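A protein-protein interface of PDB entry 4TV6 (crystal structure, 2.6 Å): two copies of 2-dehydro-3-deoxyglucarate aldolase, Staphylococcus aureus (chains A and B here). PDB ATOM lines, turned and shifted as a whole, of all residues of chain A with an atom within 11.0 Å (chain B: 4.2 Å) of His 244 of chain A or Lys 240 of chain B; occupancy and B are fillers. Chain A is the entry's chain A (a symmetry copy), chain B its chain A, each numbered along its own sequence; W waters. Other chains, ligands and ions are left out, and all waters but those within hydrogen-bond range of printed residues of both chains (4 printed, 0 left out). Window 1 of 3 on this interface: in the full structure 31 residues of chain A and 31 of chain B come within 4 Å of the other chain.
ND1 of His 244 of chain A lies within hydrogen-bond range of ND1 of His 244 of chain B (3.3 Å).
OD2 of Asp 236 of chain B is in hydrogen-bond range of N of Arg 238 of chain B, 3.4 Å away.
The side-chain hydroxyl (OG) of Ser 36 of chain A sits at hydrogen-bond distance from the backbone carbonyl oxygen (O) of Val 32 of chain A (2.9 Å).
The backbone carbonyl oxygen (O) of Ser 248 of chain A is in hydrogen-bond range of the side-chain hydroxyl (OG) of Ser 252 of chain A, 2.8 Å away.
Of the 11 printed residues of chain B, 6 touch a printed residue of chain A.
Of the 24 printed residues of chain A, 8 touch a printed residue of chain B.
Among the printed residues, 10 pairs touch across the chains.
Among the printed residues, pairs that only touch across the chains: Ile 241 of chain A with Ile 241 of chain B (3.6 Å), Ser 248 of chain A with Lys 240 of chain B (3.6 Å), Val 32 of chain A with Arg 238 of chain B (3.6 Å), Ser 252 of chain A with Leu 234 of chain B (3.6 Å), Leu 249 of chain A with Leu 234 of chain B (3.7 Å), Val 32 of chain A with Ile 241 of chain B (3.7 Å), Lys 240 of chain A with His 244 of chain B (3.9 Å), His 244 of chain A with Lys 240 of chain B (3.9 Å) and Ser 36 of chain A with Tyr 242 of chain B (3.9 Å).
Lys 240 of chain A touches His 244 of chain B, and with the chains exchanged His 244 of chain A touches Lys 240 of chain B.
Ile 241 of chain B touches its own counterpart, Ile 241 of chain A.
His 244 of chain B touches its own counterpart, His 244 of chain A.
Printed residues of chain B within 4 Å of Ile 241 of chain A: Ile 241 (3.6 Å).
Of chain B, only Lys 240 (3.9 Å) and His 244 (3.3 Å) come within 4 Å of His 244 of chain A.
Printed residues of chain B within 4 Å of Ser 248 of chain A: Lys 240 (3.6 Å).
Leu 234 of chain B touches just these residues of chain A: Leu 249 (3.7 Å) and Ser 252 (3.6 Å).
Of the printed residues of chain A, Lys 240 of chain B touches His 244 (3.9 Å) and Ser 248 (3.6 Å).
Of the printed residues of chain A, Tyr 242 of chain B touches Ser 36 (3.9 Å).
No residue of chain A comes within 4 Å of Arg 243 of chain B.
His 244 of chain B touches two residues of chain A.
The nearest printed residue of chain A that does not touch Lys 240 of chain B is Leu 245 of chain A (4.01 Å).
The nearest printed residue of chain B that does not touch Val 32 of chain A is Tyr 242 of chain B (4.4 Å).
Water W4 lies within hydrogen-bond range of OG of Ser 248 of chain A, OG of Ser 252 of chain A and NZ of Lys 240 of chain B.
Water W3 bridges a ring nitrogen (ND1) of His 244 of chain B and a ring nitrogen (ND1) of His 244 of chain A.
Water W1 bridges ND1 of His 244 of chain A (2.7 Å) and ND1 of His 244 of chain B (3.4 Å).
Water W2 bridges OG of Ser 248 of chain A (2.7 Å) and NZ of Lys 240 of chain B (2.8 Å).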
ATOM      1  N   ILE A  20      25.839  -7.427   7.820  1.00  0.00           N
ATOM      2  CA  ILE A  20      25.012  -6.825   6.784  1.00  0.00           C
ATOM      3  C   ILE A  20      23.629  -6.498   7.347  1.00  0.00           C
ATOM      4  O   ILE A  20      23.160  -7.154   8.277  1.00  0.00           O
ATOM      5  CB  ILE A  20      24.884  -7.763   5.555  1.00  0.00           C
ATOM      6  CG1 ILE A  20      24.322  -7.014   4.345  1.00  0.00           C
ATOM      7  CG2 ILE A  20      24.040  -8.988   5.888  1.00  0.00           C
ATOM      8  CD1 ILE A  20      24.151  -7.887   3.113  1.00  0.00           C
ATOM      9  N   MET A  29      16.353 -15.987   3.969  1.00  0.00           N
ATOM     10  CA  MET A  29      17.290 -14.905   3.700  1.00  0.00           C
ATOM     11  C   MET A  29      18.378 -14.867   4.767  1.00  0.00           C
ATOM     12  O   MET A  29      19.546 -14.620   4.470  1.00  0.00           O
ATOM     13  CB  MET A  29      16.564 -13.560   3.633  1.00  0.00           C
ATOM     14  CG  MET A  29      17.481 -12.382   3.361  1.00  0.00           C
ATOM     15  SD  MET A  29      18.490 -12.605   1.883  1.00  0.00           S
ATOM     16  CE  MET A  29      17.222 -12.861   0.650  1.00  0.00           C
ATOM     17  N   VAL A  32      20.684 -17.667   4.083  1.00  0.00           N
ATOM     18  CA  VAL A  32      21.471 -17.333   2.899  1.00  0.00           C
ATOM     19  C   VAL A  32      22.645 -16.431   3.278  1.00  0.00           C
ATOM     20  O   VAL A  32      23.770 -16.624   2.809  1.00  0.00           O
ATOM     21  CB  VAL A  32      20.600 -16.646   1.820  1.00  0.00           C
ATOM     22  CG1 VAL A  32      21.442 -15.765   0.905  1.00  0.00           C
ATOM     23  CG2 VAL A  32      19.836 -17.684   1.018  1.00  0.00           C
ATOM     24  N   ILE A  33      22.374 -15.452   4.135  1.00  0.00           N
ATOM     25  CA  ILE A  33      23.406 -14.545   4.624  1.00  0.00           C
ATOM     26  C   ILE A  33      24.484 -15.304   5.399  1.00  0.00           C
ATOM     27  O   ILE A  33      25.678 -15.085   5.198  1.00  0.00           O
ATOM     28  CB  ILE A  33      22.803 -13.441   5.519  1.00  0.00           C
ATOM     29  CG1 ILE A  33      21.901 -12.522   4.690  1.00  0.00           C
ATOM     30  CG2 ILE A  33      23.899 -12.628   6.182  1.00  0.00           C
ATOM     31  CD1 ILE A  33      21.021 -11.614   5.517  1.00  0.00           C
ATOM     32  N   SER A  36      26.756 -17.155   3.222  1.00  0.00           N
ATOM     33  CA  SER A  36      27.610 -16.277   2.429  1.00  0.00           C
ATOM     34  C   SER A  36      28.902 -15.938   3.169  1.00  0.00           C
ATOM     35  O   SER A  36      29.838 -15.400   2.580  1.00  0.00           O
ATOM     36  CB  SER A  36      26.863 -14.995   2.057  1.00  0.00           C
ATOM     37  OG  SER A  36      25.771 -15.277   1.198  1.00  0.00           O
ATOM     38  N   ARG A 216      31.424   2.575   2.051  1.00  0.00           N
ATOM     39  CA  ARG A 216      30.713   2.605   0.779  1.00  0.00           C
ATOM     40  C   ARG A 216      31.531   1.865  -0.279  1.00  0.00           C
ATOM     41  O   ARG A 216      30.984   1.230  -1.187  1.00  0.00           O
ATOM     42  CB  ARG A 216      30.433   4.043   0.348  1.00  0.00           C
ATOM     43  CG  ARG A 216      29.735   4.132  -0.988  1.00  0.00           C
ATOM     44  CD  ARG A 216      28.376   3.429  -0.960  1.00  0.00           C
ATOM     45  NE  ARG A 216      27.644   3.628  -2.210  1.00  0.00           N
ATOM     46  CZ  ARG A 216      26.570   2.933  -2.578  1.00  0.00           C
ATOM     47  NH1 ARG A 216      26.092   1.977  -1.792  1.00  0.00           N
ATOM     48  NH2 ARG A 216      25.971   3.189  -3.737  1.00  0.00           N
ATOM     49  N   ASP A 236      23.074  -3.358   2.865  1.00  0.00           N
ATOM     50  CA  ASP A 236      21.893  -4.134   3.221  1.00  0.00           C
ATOM     51  C   ASP A 236      21.585  -5.152   2.130  1.00  0.00           C
ATOM     52  O   ASP A 236      21.890  -4.921   0.960  1.00  0.00           O
ATOM     53  CB  ASP A 236      20.690  -3.217   3.455  1.00  0.00           C
ATOM     54  CG  ASP A 236      20.128  -2.649   2.169  1.00  0.00           C
ATOM     55  OD1 ASP A 236      20.784  -1.771   1.568  1.00  0.00           O
ATOM     56  OD2 ASP A 236      19.024  -3.073   1.766  1.00  0.00           O
ATOM     57  N   ASP A 237      20.981  -6.273   2.518  1.00  0.00           N
ATOM     58  CA  ASP A 237      20.716  -7.361   1.582  1.00  0.00           C
ATOM     59  C   ASP A 237      19.856  -6.907   0.405  1.00  0.00           C
ATOM     60  O   ASP A 237      20.217  -7.121  -0.749  1.00  0.00           O
ATOM     61  CB  ASP A 237      20.053  -8.545   2.298  1.00  0.00           C
ATOM     62  CG  ASP A 237      18.846  -8.138   3.126  1.00  0.00           C
ATOM     63  OD1 ASP A 237      18.382  -6.985   3.001  1.00  0.00           O
ATOM     64  OD2 ASP A 237      18.355  -8.986   3.901  1.00  0.00           O
ATOM     65  N   ARG A 238      18.733  -6.264   0.706  1.00  0.00           N
ATOM     66  CA  ARG A 238      17.807  -5.793  -0.318  1.00  0.00           C
ATOM     67  C   ARG A 238      18.493  -4.875  -1.326  1.00  0.00           C
ATOM     68  O   ARG A 238      18.227  -4.948  -2.526  1.00  0.00           O
ATOM     69  CB  ARG A 238      16.624  -5.073   0.333  1.00  0.00           C
ATOM     70  CG  ARG A 238      15.524  -4.678  -0.634  1.00  0.00           C
ATOM     71  CD  ARG A 238      14.238  -4.343   0.104  1.00  0.00           C
ATOM     72  NE  ARG A 238      14.409  -3.237   1.042  1.00  0.00           N
ATOM     73  CZ  ARG A 238      13.452  -2.785   1.845  1.00  0.00           C
ATOM     74  NH1 ARG A 238      12.252  -3.345   1.829  1.00  0.00           N
ATOM     75  NH2 ARG A 238      13.695  -1.773   2.668  1.00  0.00           N
ATOM     76  N   GLY A 239      19.385  -4.022  -0.831  1.00  0.00           N
ATOM     77  CA  GLY A 239      20.112  -3.098  -1.682  1.00  0.00           C
ATOM     78  C   GLY A 239      21.086  -3.792  -2.615  1.00  0.00           C
ATOM     79  O   GLY A 239      21.157  -3.471  -3.800  1.00  0.00           O
ATOM     80  N   LYS A 240      21.840  -4.748  -2.081  1.00  0.00           N
ATOM     81  CA  LYS A 240      22.819  -5.479  -2.877  1.00  0.00           C
ATOM     82  C   LYS A 240      22.154  -6.446  -3.853  1.00  0.00           C
ATOM     83  O   LYS A 240      22.666  -6.689  -4.944  1.00  0.00           O
ATOM     84  CB  LYS A 240      23.787  -6.241  -1.968  1.00  0.00           C
ATOM     85  CG  LYS A 240      24.740  -5.352  -1.194  1.00  0.00           C
ATOM     86  CD  LYS A 240      25.548  -6.158  -0.194  1.00  0.00           C
ATOM     87  CE  LYS A 240      26.905  -5.524   0.059  1.00  0.00           C
ATOM     88  NZ  LYS A 240      27.745  -5.515  -1.170  1.00  0.00           N
ATOM     89  N   ILE A 241      21.013  -6.999  -3.456  1.00  0.00           N
ATOM     90  CA  ILE A 241      20.293  -7.946  -4.299  1.00  0.00           C
ATOM     91  C   ILE A 241      19.682  -7.243  -5.509  1.00  0.00           C
ATOM     92  O   ILE A 241      19.722  -7.768  -6.622  1.00  0.00           O
ATOM     93  CB  ILE A 241      19.196  -8.681  -3.501  1.00  0.00           C
ATOM     94  CG1 ILE A 241      19.836  -9.637  -2.493  1.00  0.00           C
ATOM     95  CG2 ILE A 241      18.273  -9.456  -4.427  1.00  0.00           C
ATOM     96  CD1 ILE A 241      18.875 -10.147  -1.439  1.00  0.00           C
ATOM     97  N   TYR A 242      19.134  -6.050  -5.295  1.00  0.00           N
ATOM     98  CA  TYR A 242      18.596  -5.261  -6.399  1.00  0.00           C
ATOM     99  C   TYR A 242      19.692  -4.875  -7.385  1.00  0.00           C
ATOM    100  O   TYR A 242      19.503  -4.953  -8.600  1.00  0.00           O
ATOM    101  CB  TYR A 242      17.901  -3.997  -5.886  1.00  0.00           C
ATOM    102  CG  TYR A 242      17.689  -2.958  -6.968  1.00  0.00           C
ATOM    103  CD1 TYR A 242      16.659  -3.088  -7.891  1.00  0.00           C
ATOM    104  CD2 TYR A 242      18.525  -1.852  -7.071  1.00  0.00           C
ATOM    105  CE1 TYR A 242      16.466  -2.148  -8.885  1.00  0.00           C
ATOM    106  CE2 TYR A 242      18.340  -0.907  -8.062  1.00  0.00           C
ATOM    107  CZ  TYR A 242      17.308  -1.058  -8.965  1.00  0.00           C
ATOM    108  OH  TYR A 242      17.120  -0.118  -9.953  1.00  0.00           O
ATOM    109  N   ARG A 243      20.836  -4.454  -6.855  1.00  0.00           N
ATOM    110  CA  ARG A 243      21.943  -4.004  -7.688  1.00  0.00           C
ATOM    111  C   ARG A 243      22.509  -5.135  -8.542  1.00  0.00           C
ATOM    112  O   ARG A 243      22.758  -4.953  -9.733  1.00  0.00           O
ATOM    113  CB  ARG A 243      23.047  -3.390  -6.825  1.00  0.00           C
ATOM    114  CG  ARG A 243      22.729  -1.981  -6.349  1.00  0.00           C
ATOM    115  CD  ARG A 243      23.951  -1.288  -5.764  1.00  0.00           C
ATOM    116  NE  ARG A 243      24.304  -1.806  -4.445  1.00  0.00           N
ATOM    117  CZ  ARG A 243      23.706  -1.442  -3.315  1.00  0.00           C
ATOM    118  NH1 ARG A 243      22.716  -0.558  -3.342  1.00  0.00           N
ATOM    119  NH2 ARG A 243      24.094  -1.963  -2.159  1.00  0.00           N
ATOM    120  N   HIS A 244      22.706  -6.301  -7.936  1.00  0.00           N
ATOM    121  CA  HIS A 244      23.237  -7.444  -8.669  1.00  0.00           C
ATOM    122  C   HIS A 244      22.251  -7.944  -9.721  1.00  0.00           C
ATOM    123  O   HIS A 244      22.619  -8.146 -10.879  1.00  0.00           O
ATOM    124  CB  HIS A 244      23.596  -8.586  -7.716  1.00  0.00           C
ATOM    125  CG  HIS A 244      24.051  -9.831  -8.417  1.00  0.00           C
ATOM    126  ND1 HIS A 244      25.213  -9.888  -9.153  1.00  0.00           N
ATOM    127  CD2 HIS A 244      23.489 -11.061  -8.504  1.00  0.00           C
ATOM    128  CE1 HIS A 244      25.354 -11.102  -9.660  1.00  0.00           C
ATOM    129  NE2 HIS A 244      24.321 -11.832  -9.281  1.00  0.00           N
ATOM    130  N   LEU A 245      21.001  -8.137  -9.312  1.00  0.00           N
ATOM    131  CA  LEU A 245      19.977  -8.703 -10.186  1.00  0.00           C
ATOM    132  C   LEU A 245      19.683  -7.838 -11.409  1.00  0.00           C
ATOM    133  O   LEU A 245      19.685  -8.332 -12.536  1.00  0.00           O
ATOM    134  CB  LEU A 245      18.682  -8.934  -9.404  1.00  0.00           C
ATOM    135  CG  LEU A 245      18.585 -10.251  -8.633  1.00  0.00           C
ATOM    136  CD1 LEU A 245      17.246 -10.362  -7.922  1.00  0.00           C
ATOM    137  CD2 LEU A 245      18.796 -11.430  -9.572  1.00  0.00           C
ATOM    138  N   SER A 246      19.424  -6.553 -11.183  1.00  0.00           N
ATOM    139  CA  SER A 246      19.066  -5.642 -12.266  1.00  0.00           C
ATOM    140  C   SER A 246      20.203  -5.497 -13.273  1.00  0.00           C
ATOM    141  O   SER A 246      19.969  -5.398 -14.478  1.00  0.00           O
ATOM    142  CB  SER A 246      18.679  -4.269 -11.710  1.00  0.00           C
ATOM    143  OG  SER A 246      19.761  -3.674 -11.016  1.00  0.00           O
ATOM    144  N   ALA A 247      21.433  -5.493 -12.771  1.00  0.00           N
ATOM    145  CA  ALA A 247      22.607  -5.379 -13.629  1.00  0.00           C
ATOM    146  C   ALA A 247      22.853  -6.672 -14.401  1.00  0.00           C
ATOM    147  O   ALA A 247      23.108  -6.644 -15.604  1.00  0.00           O
ATOM    148  CB  ALA A 247      23.831  -5.013 -12.806  1.00  0.00           C
ATOM    149  N   SER A 248      22.778  -7.800 -13.700  1.00  0.00           N
ATOM    150  CA  SER A 248      22.988  -9.104 -14.318  1.00  0.00           C
ATOM    151  C   SER A 248      21.964  -9.363 -15.419  1.00  0.00           C
ATOM    152  O   SER A 248      22.297  -9.901 -16.475  1.00  0.00           O
ATOM    153  CB  SER A 248      22.917 -10.214 -13.268  1.00  0.00           C
ATOM    154  OG  SER A 248      23.001 -11.491 -13.874  1.00  0.00           O
ATOM    155  N   LEU A 249      20.720  -8.973 -15.163  1.00  0.00           N
ATOM    156  CA  LEU A 249      19.657  -9.110 -16.149  1.00  0.00           C
ATOM    157  C   LEU A 249      19.908  -8.199 -17.345  1.00  0.00           C
ATOM    158  O   LEU A 249      19.644  -8.574 -18.488  1.00  0.00           O
ATOM    159  CB  LEU A 249      18.298  -8.796 -15.522  1.00  0.00           C
ATOM    160  CG  LEU A 249      17.097  -8.823 -16.472  1.00  0.00           C
ATOM    161  CD1 LEU A 249      16.891 -10.214 -17.046  1.00  0.00           C
ATOM    162  CD2 LEU A 249      15.848  -8.339 -15.764  1.00  0.00           C
ATOM    163  N   ALA A 250      20.419  -7.001 -17.074  1.00  0.00           N
ATOM    164  CA  ALA A 250      20.724  -6.037 -18.127  1.00  0.00           C
ATOM    165  C   ALA A 250      21.781  -6.587 -19.078  1.00  0.00           C
ATOM    166  O   ALA A 250      21.648  -6.485 -20.299  1.00  0.00           O
ATOM    167  CB  ALA A 250      21.182  -4.718 -17.526  1.00  0.00           C
ATOM    168  N   THR A 251      22.828  -7.173 -18.505  1.00  0.00           N
ATOM    169  CA  THR A 251      23.882  -7.806 -19.284  1.00  0.00           C
ATOM    170  C   THR A 251      23.325  -8.996 -20.067  1.00  0.00           C
ATOM    171  O   THR A 251      23.762  -9.272 -21.183  1.00  0.00           O
ATOM    172  CB  THR A 251      25.044  -8.276 -18.381  1.00  0.00           C
ATOM    173  OG1 THR A 251      25.552  -7.160 -17.641  1.00  0.00           O
ATOM    174  CG2 THR A 251      26.169  -8.879 -19.212  1.00  0.00           C
ATOM    175  N   SER A 252      22.347  -9.686 -19.478  1.00  0.00           N
ATOM    176  CA  SER A 252      21.734 -10.857 -20.103  1.00  0.00           C
ATOM    177  C   SER A 252      21.017 -10.482 -21.395  1.00  0.00           C
ATOM    178  O   SER A 252      21.041 -11.235 -22.371  1.00  0.00           O
ATOM    179  CB  SER A 252      20.756 -11.537 -19.141  1.00  0.00           C
ATOM    180  OG  SER A 252      21.423 -12.048 -18.003  1.00  0.00           O
ATOM    181  N   LYS A 253      20.372  -9.320 -21.400  1.00  0.00           N
ATOM    182  CA  LYS A 253      19.713  -8.828 -22.605  1.00  0.00           C
ATOM    183  C   LYS A 253      20.756  -8.282 -23.572  1.00  0.00           C
ATOM    184  O   LYS A 253      20.662  -8.482 -24.784  1.00  0.00           O
ATOM    185  CB  LYS A 253      18.689  -7.750 -22.255  1.00  0.00           C
ATOM    186  CG  LYS A 253      17.610  -8.210 -21.290  1.00  0.00           C
ATOM    187  CD  LYS A 253      16.605  -7.110 -21.018  1.00  0.00           C
ATOM    188  CE  LYS A 253      15.497  -7.580 -20.099  1.00  0.00           C
ATOM    189  NZ  LYS A 253      14.502  -6.499 -19.878  1.00  0.00           N
ATOM    190  N   ILE B  20      12.608 -15.549 -13.520  1.00  0.00           N
ATOM    191  CA  ILE B  20      13.516 -16.130 -12.541  1.00  0.00           C
ATOM    192  C   ILE B  20      12.732 -16.997 -11.556  1.00  0.00           C
ATOM    193  O   ILE B  20      11.552 -16.752 -11.306  1.00  0.00           O
ATOM    194  CB  ILE B  20      14.300 -15.029 -11.782  1.00  0.00           C
ATOM    195  CG1 ILE B  20      15.485 -15.622 -11.017  1.00  0.00           C
ATOM    196  CG2 ILE B  20      13.381 -14.243 -10.854  1.00  0.00           C
ATOM    197  CD1 ILE B  20      16.282 -14.593 -10.233  1.00  0.00           C
ATOM    198  N   LEU B 234      16.182 -17.260 -15.949  1.00  0.00           N
ATOM    199  CA  LEU B 234      17.580 -17.096 -15.569  1.00  0.00           C
ATOM    200  C   LEU B 234      17.820 -17.462 -14.107  1.00  0.00           C
ATOM    201  O   LEU B 234      17.882 -16.588 -13.244  1.00  0.00           O
ATOM    202  CB  LEU B 234      18.033 -15.658 -15.829  1.00  0.00           C
ATOM    203  CG  LEU B 234      17.711 -15.078 -17.209  1.00  0.00           C
ATOM    204  CD1 LEU B 234      18.222 -13.648 -17.321  1.00  0.00           C
ATOM    205  CD2 LEU B 234      18.291 -15.945 -18.316  1.00  0.00           C
ATOM    206  N   ASP B 236      17.650 -19.049 -10.193  1.00  0.00           N
ATOM    207  CA  ASP B 236      16.760 -18.789  -9.068  1.00  0.00           C
ATOM    208  C   ASP B 236      17.346 -17.703  -8.175  1.00  0.00           C
ATOM    209  O   ASP B 236      18.565 -17.554  -8.095  1.00  0.00           O
ATOM    210  CB  ASP B 236      16.512 -20.068  -8.265  1.00  0.00           C
ATOM    211  CG  ASP B 236      17.709 -20.478  -7.432  1.00  0.00           C
ATOM    212  OD1 ASP B 236      18.711 -20.943  -8.017  1.00  0.00           O
ATOM    213  OD2 ASP B 236      17.641 -20.346  -6.191  1.00  0.00           O
ATOM    214  N   ASP B 237      16.475 -16.950  -7.509  1.00  0.00           N
ATOM    215  CA  ASP B 237      16.908 -15.819  -6.693  1.00  0.00           C
ATOM    216  C   ASP B 237      17.888 -16.244  -5.603  1.00  0.00           C
ATOM    217  O   ASP B 237      18.968 -15.670  -5.477  1.00  0.00           O
ATOM    218  CB  ASP B 237      15.703 -15.101  -6.074  1.00  0.00           C
ATOM    219  CG  ASP B 237      14.751 -16.046  -5.358  1.00  0.00           C
ATOM    220  OD1 ASP B 237      15.105 -17.227  -5.154  1.00  0.00           O
ATOM    221  OD2 ASP B 237      13.645 -15.596  -4.992  1.00  0.00           O
ATOM    222  N   ARG B 238      17.514 -17.260  -4.833  1.00  0.00           N
ATOM    223  CA  ARG B 238      18.343 -17.755  -3.739  1.00  0.00           C
ATOM    224  C   ARG B 238      19.736 -18.154  -4.218  1.00  0.00           C
ATOM    225  O   ARG B 238      20.731 -17.900  -3.539  1.00  0.00           O
ATOM    226  CB  ARG B 238      17.659 -18.941  -3.055  1.00  0.00           C
ATOM    227  CG  ARG B 238      18.365 -19.434  -1.807  1.00  0.00           C
ATOM    228  CD  ARG B 238      17.451 -20.317  -0.972  1.00  0.00           C
ATOM    229  NE  ARG B 238      16.995 -21.494  -1.707  1.00  0.00           N
ATOM    230  CZ  ARG B 238      16.149 -22.396  -1.221  1.00  0.00           C
ATOM    231  NH1 ARG B 238      15.661 -22.257   0.003  1.00  0.00           N
ATOM    232  NH2 ARG B 238      15.788 -23.437  -1.959  1.00  0.00           N
ATOM    233  N   GLY B 239      19.799 -18.770  -5.395  1.00  0.00           N
ATOM    234  CA  GLY B 239      21.062 -19.197  -5.968  1.00  0.00           C
ATOM    235  C   GLY B 239      21.954 -18.038  -6.368  1.00  0.00           C
ATOM    236  O   GLY B 239      23.152 -18.043  -6.090  1.00  0.00           O
ATOM    237  N   LYS B 240      21.370 -17.040  -7.024  1.00  0.00           N
ATOM    238  CA  LYS B 240      22.128 -15.876  -7.469  1.00  0.00           C
ATOM    239  C   LYS B 240      22.528 -14.975  -6.304  1.00  0.00           C
ATOM    240  O   LYS B 240      23.582 -14.342  -6.332  1.00  0.00           O
ATOM    241  CB  LYS B 240      21.323 -15.074  -8.494  1.00  0.00           C
ATOM    242  CG  LYS B 240      21.160 -15.766  -9.834  1.00  0.00           C
ATOM    243  CD  LYS B 240      20.214 -14.994 -10.735  1.00  0.00           C
ATOM    244  CE  LYS B 240      20.553 -15.205 -12.201  1.00  0.00           C
ATOM    245  NZ  LYS B 240      21.901 -14.668 -12.536  1.00  0.00           N
ATOM    246  N   ILE B 241      21.683 -14.917  -5.281  1.00  0.00           N
ATOM    247  CA  ILE B 241      21.953 -14.082  -4.116  1.00  0.00           C
ATOM    248  C   ILE B 241      23.110 -14.649  -3.297  1.00  0.00           C
ATOM    249  O   ILE B 241      23.966 -13.901  -2.825  1.00  0.00           O
ATOM    250  CB  ILE B 241      20.697 -13.934  -3.233  1.00  0.00           C
ATOM    251  CG1 ILE B 241      19.651 -13.079  -3.951  1.00  0.00           C
ATOM    252  CG2 ILE B 241      21.043 -13.303  -1.894  1.00  0.00           C
ATOM    253  CD1 ILE B 241      18.271 -13.152  -3.331  1.00  0.00           C
ATOM    254  N   TYR B 242      23.145 -15.970  -3.144  1.00  0.00           N
ATOM    255  CA  TYR B 242      24.252 -16.617  -2.448  1.00  0.00           C
ATOM    256  C   TYR B 242      25.568 -16.401  -3.186  1.00  0.00           C
ATOM    257  O   TYR B 242      26.596 -16.115  -2.571  1.00  0.00           O
ATOM    258  CB  TYR B 242      23.999 -18.118  -2.281  1.00  0.00           C
ATOM    259  CG  TYR B 242      25.253 -18.896  -1.945  1.00  0.00           C
ATOM    260  CD1 TYR B 242      25.772 -18.894  -0.656  1.00  0.00           C
ATOM    261  CD2 TYR B 242      25.924 -19.627  -2.920  1.00  0.00           C
ATOM    262  CE1 TYR B 242      26.920 -19.596  -0.346  1.00  0.00           C
ATOM    263  CE2 TYR B 242      27.074 -20.331  -2.618  1.00  0.00           C
ATOM    264  CZ  TYR B 242      27.567 -20.315  -1.330  1.00  0.00           C
ATOM    265  OH  TYR B 242      28.711 -21.016  -1.027  1.00  0.00           O
ATOM    266  N   ARG B 243      25.530 -16.547  -4.506  1.00  0.00           N
ATOM    267  CA  ARG B 243      26.730 -16.422  -5.322  1.00  0.00           C
ATOM    268  C   ARG B 243      27.301 -15.007  -5.282  1.00  0.00           C
ATOM    269  O   ARG B 243      28.509 -14.827  -5.132  1.00  0.00           O
ATOM    270  CB  ARG B 243      26.439 -16.833  -6.767  1.00  0.00           C
ATOM    271  CG  ARG B 243      26.368 -18.340  -6.965  1.00  0.00           C
ATOM    272  CD  ARG B 243      26.387 -18.723  -8.437  1.00  0.00           C
ATOM    273  NE  ARG B 243      25.120 -18.433  -9.102  1.00  0.00           N
ATOM    274  CZ  ARG B 243      24.046 -19.214  -9.037  1.00  0.00           C
ATOM    275  NH1 ARG B 243      24.082 -20.335  -8.328  1.00  0.00           N
ATOM    276  NH2 ARG B 243      22.935 -18.873  -9.676  1.00  0.00           N
ATOM    277  N   HIS B 244      26.434 -14.009  -5.409  1.00  0.00           N
ATOM    278  CA  HIS B 244      26.882 -12.621  -5.376  1.00  0.00           C
ATOM    279  C   HIS B 244      27.413 -12.235  -3.997  1.00  0.00           C
ATOM    280  O   HIS B 244      28.500 -11.670  -3.880  1.00  0.00           O
ATOM    281  CB  HIS B 244      25.752 -11.672  -5.777  1.00  0.00           C
ATOM    282  CG  HIS B 244      26.118 -10.222  -5.663  1.00  0.00           C
ATOM    283  ND1 HIS B 244      27.084  -9.634  -6.448  1.00  0.00           N
ATOM    284  CD2 HIS B 244      25.654  -9.248  -4.843  1.00  0.00           C
ATOM    285  CE1 HIS B 244      27.197  -8.357  -6.123  1.00  0.00           C
ATOM    286  NE2 HIS B 244      26.342  -8.098  -5.153  1.00  0.00           N
HETATM  287  O   HOH W   1      26.747  -7.629  -9.212  1.00  0.00           O
HETATM  288  O   HOH W   2      24.311 -13.898 -13.845  1.00  0.00           O
HETATM  289  O   HOH W   3      28.269 -11.216  -8.334  1.00  0.00           O
HETATM  290  O   HOH W   4      21.005 -12.711 -15.048  1.00  0.00           O
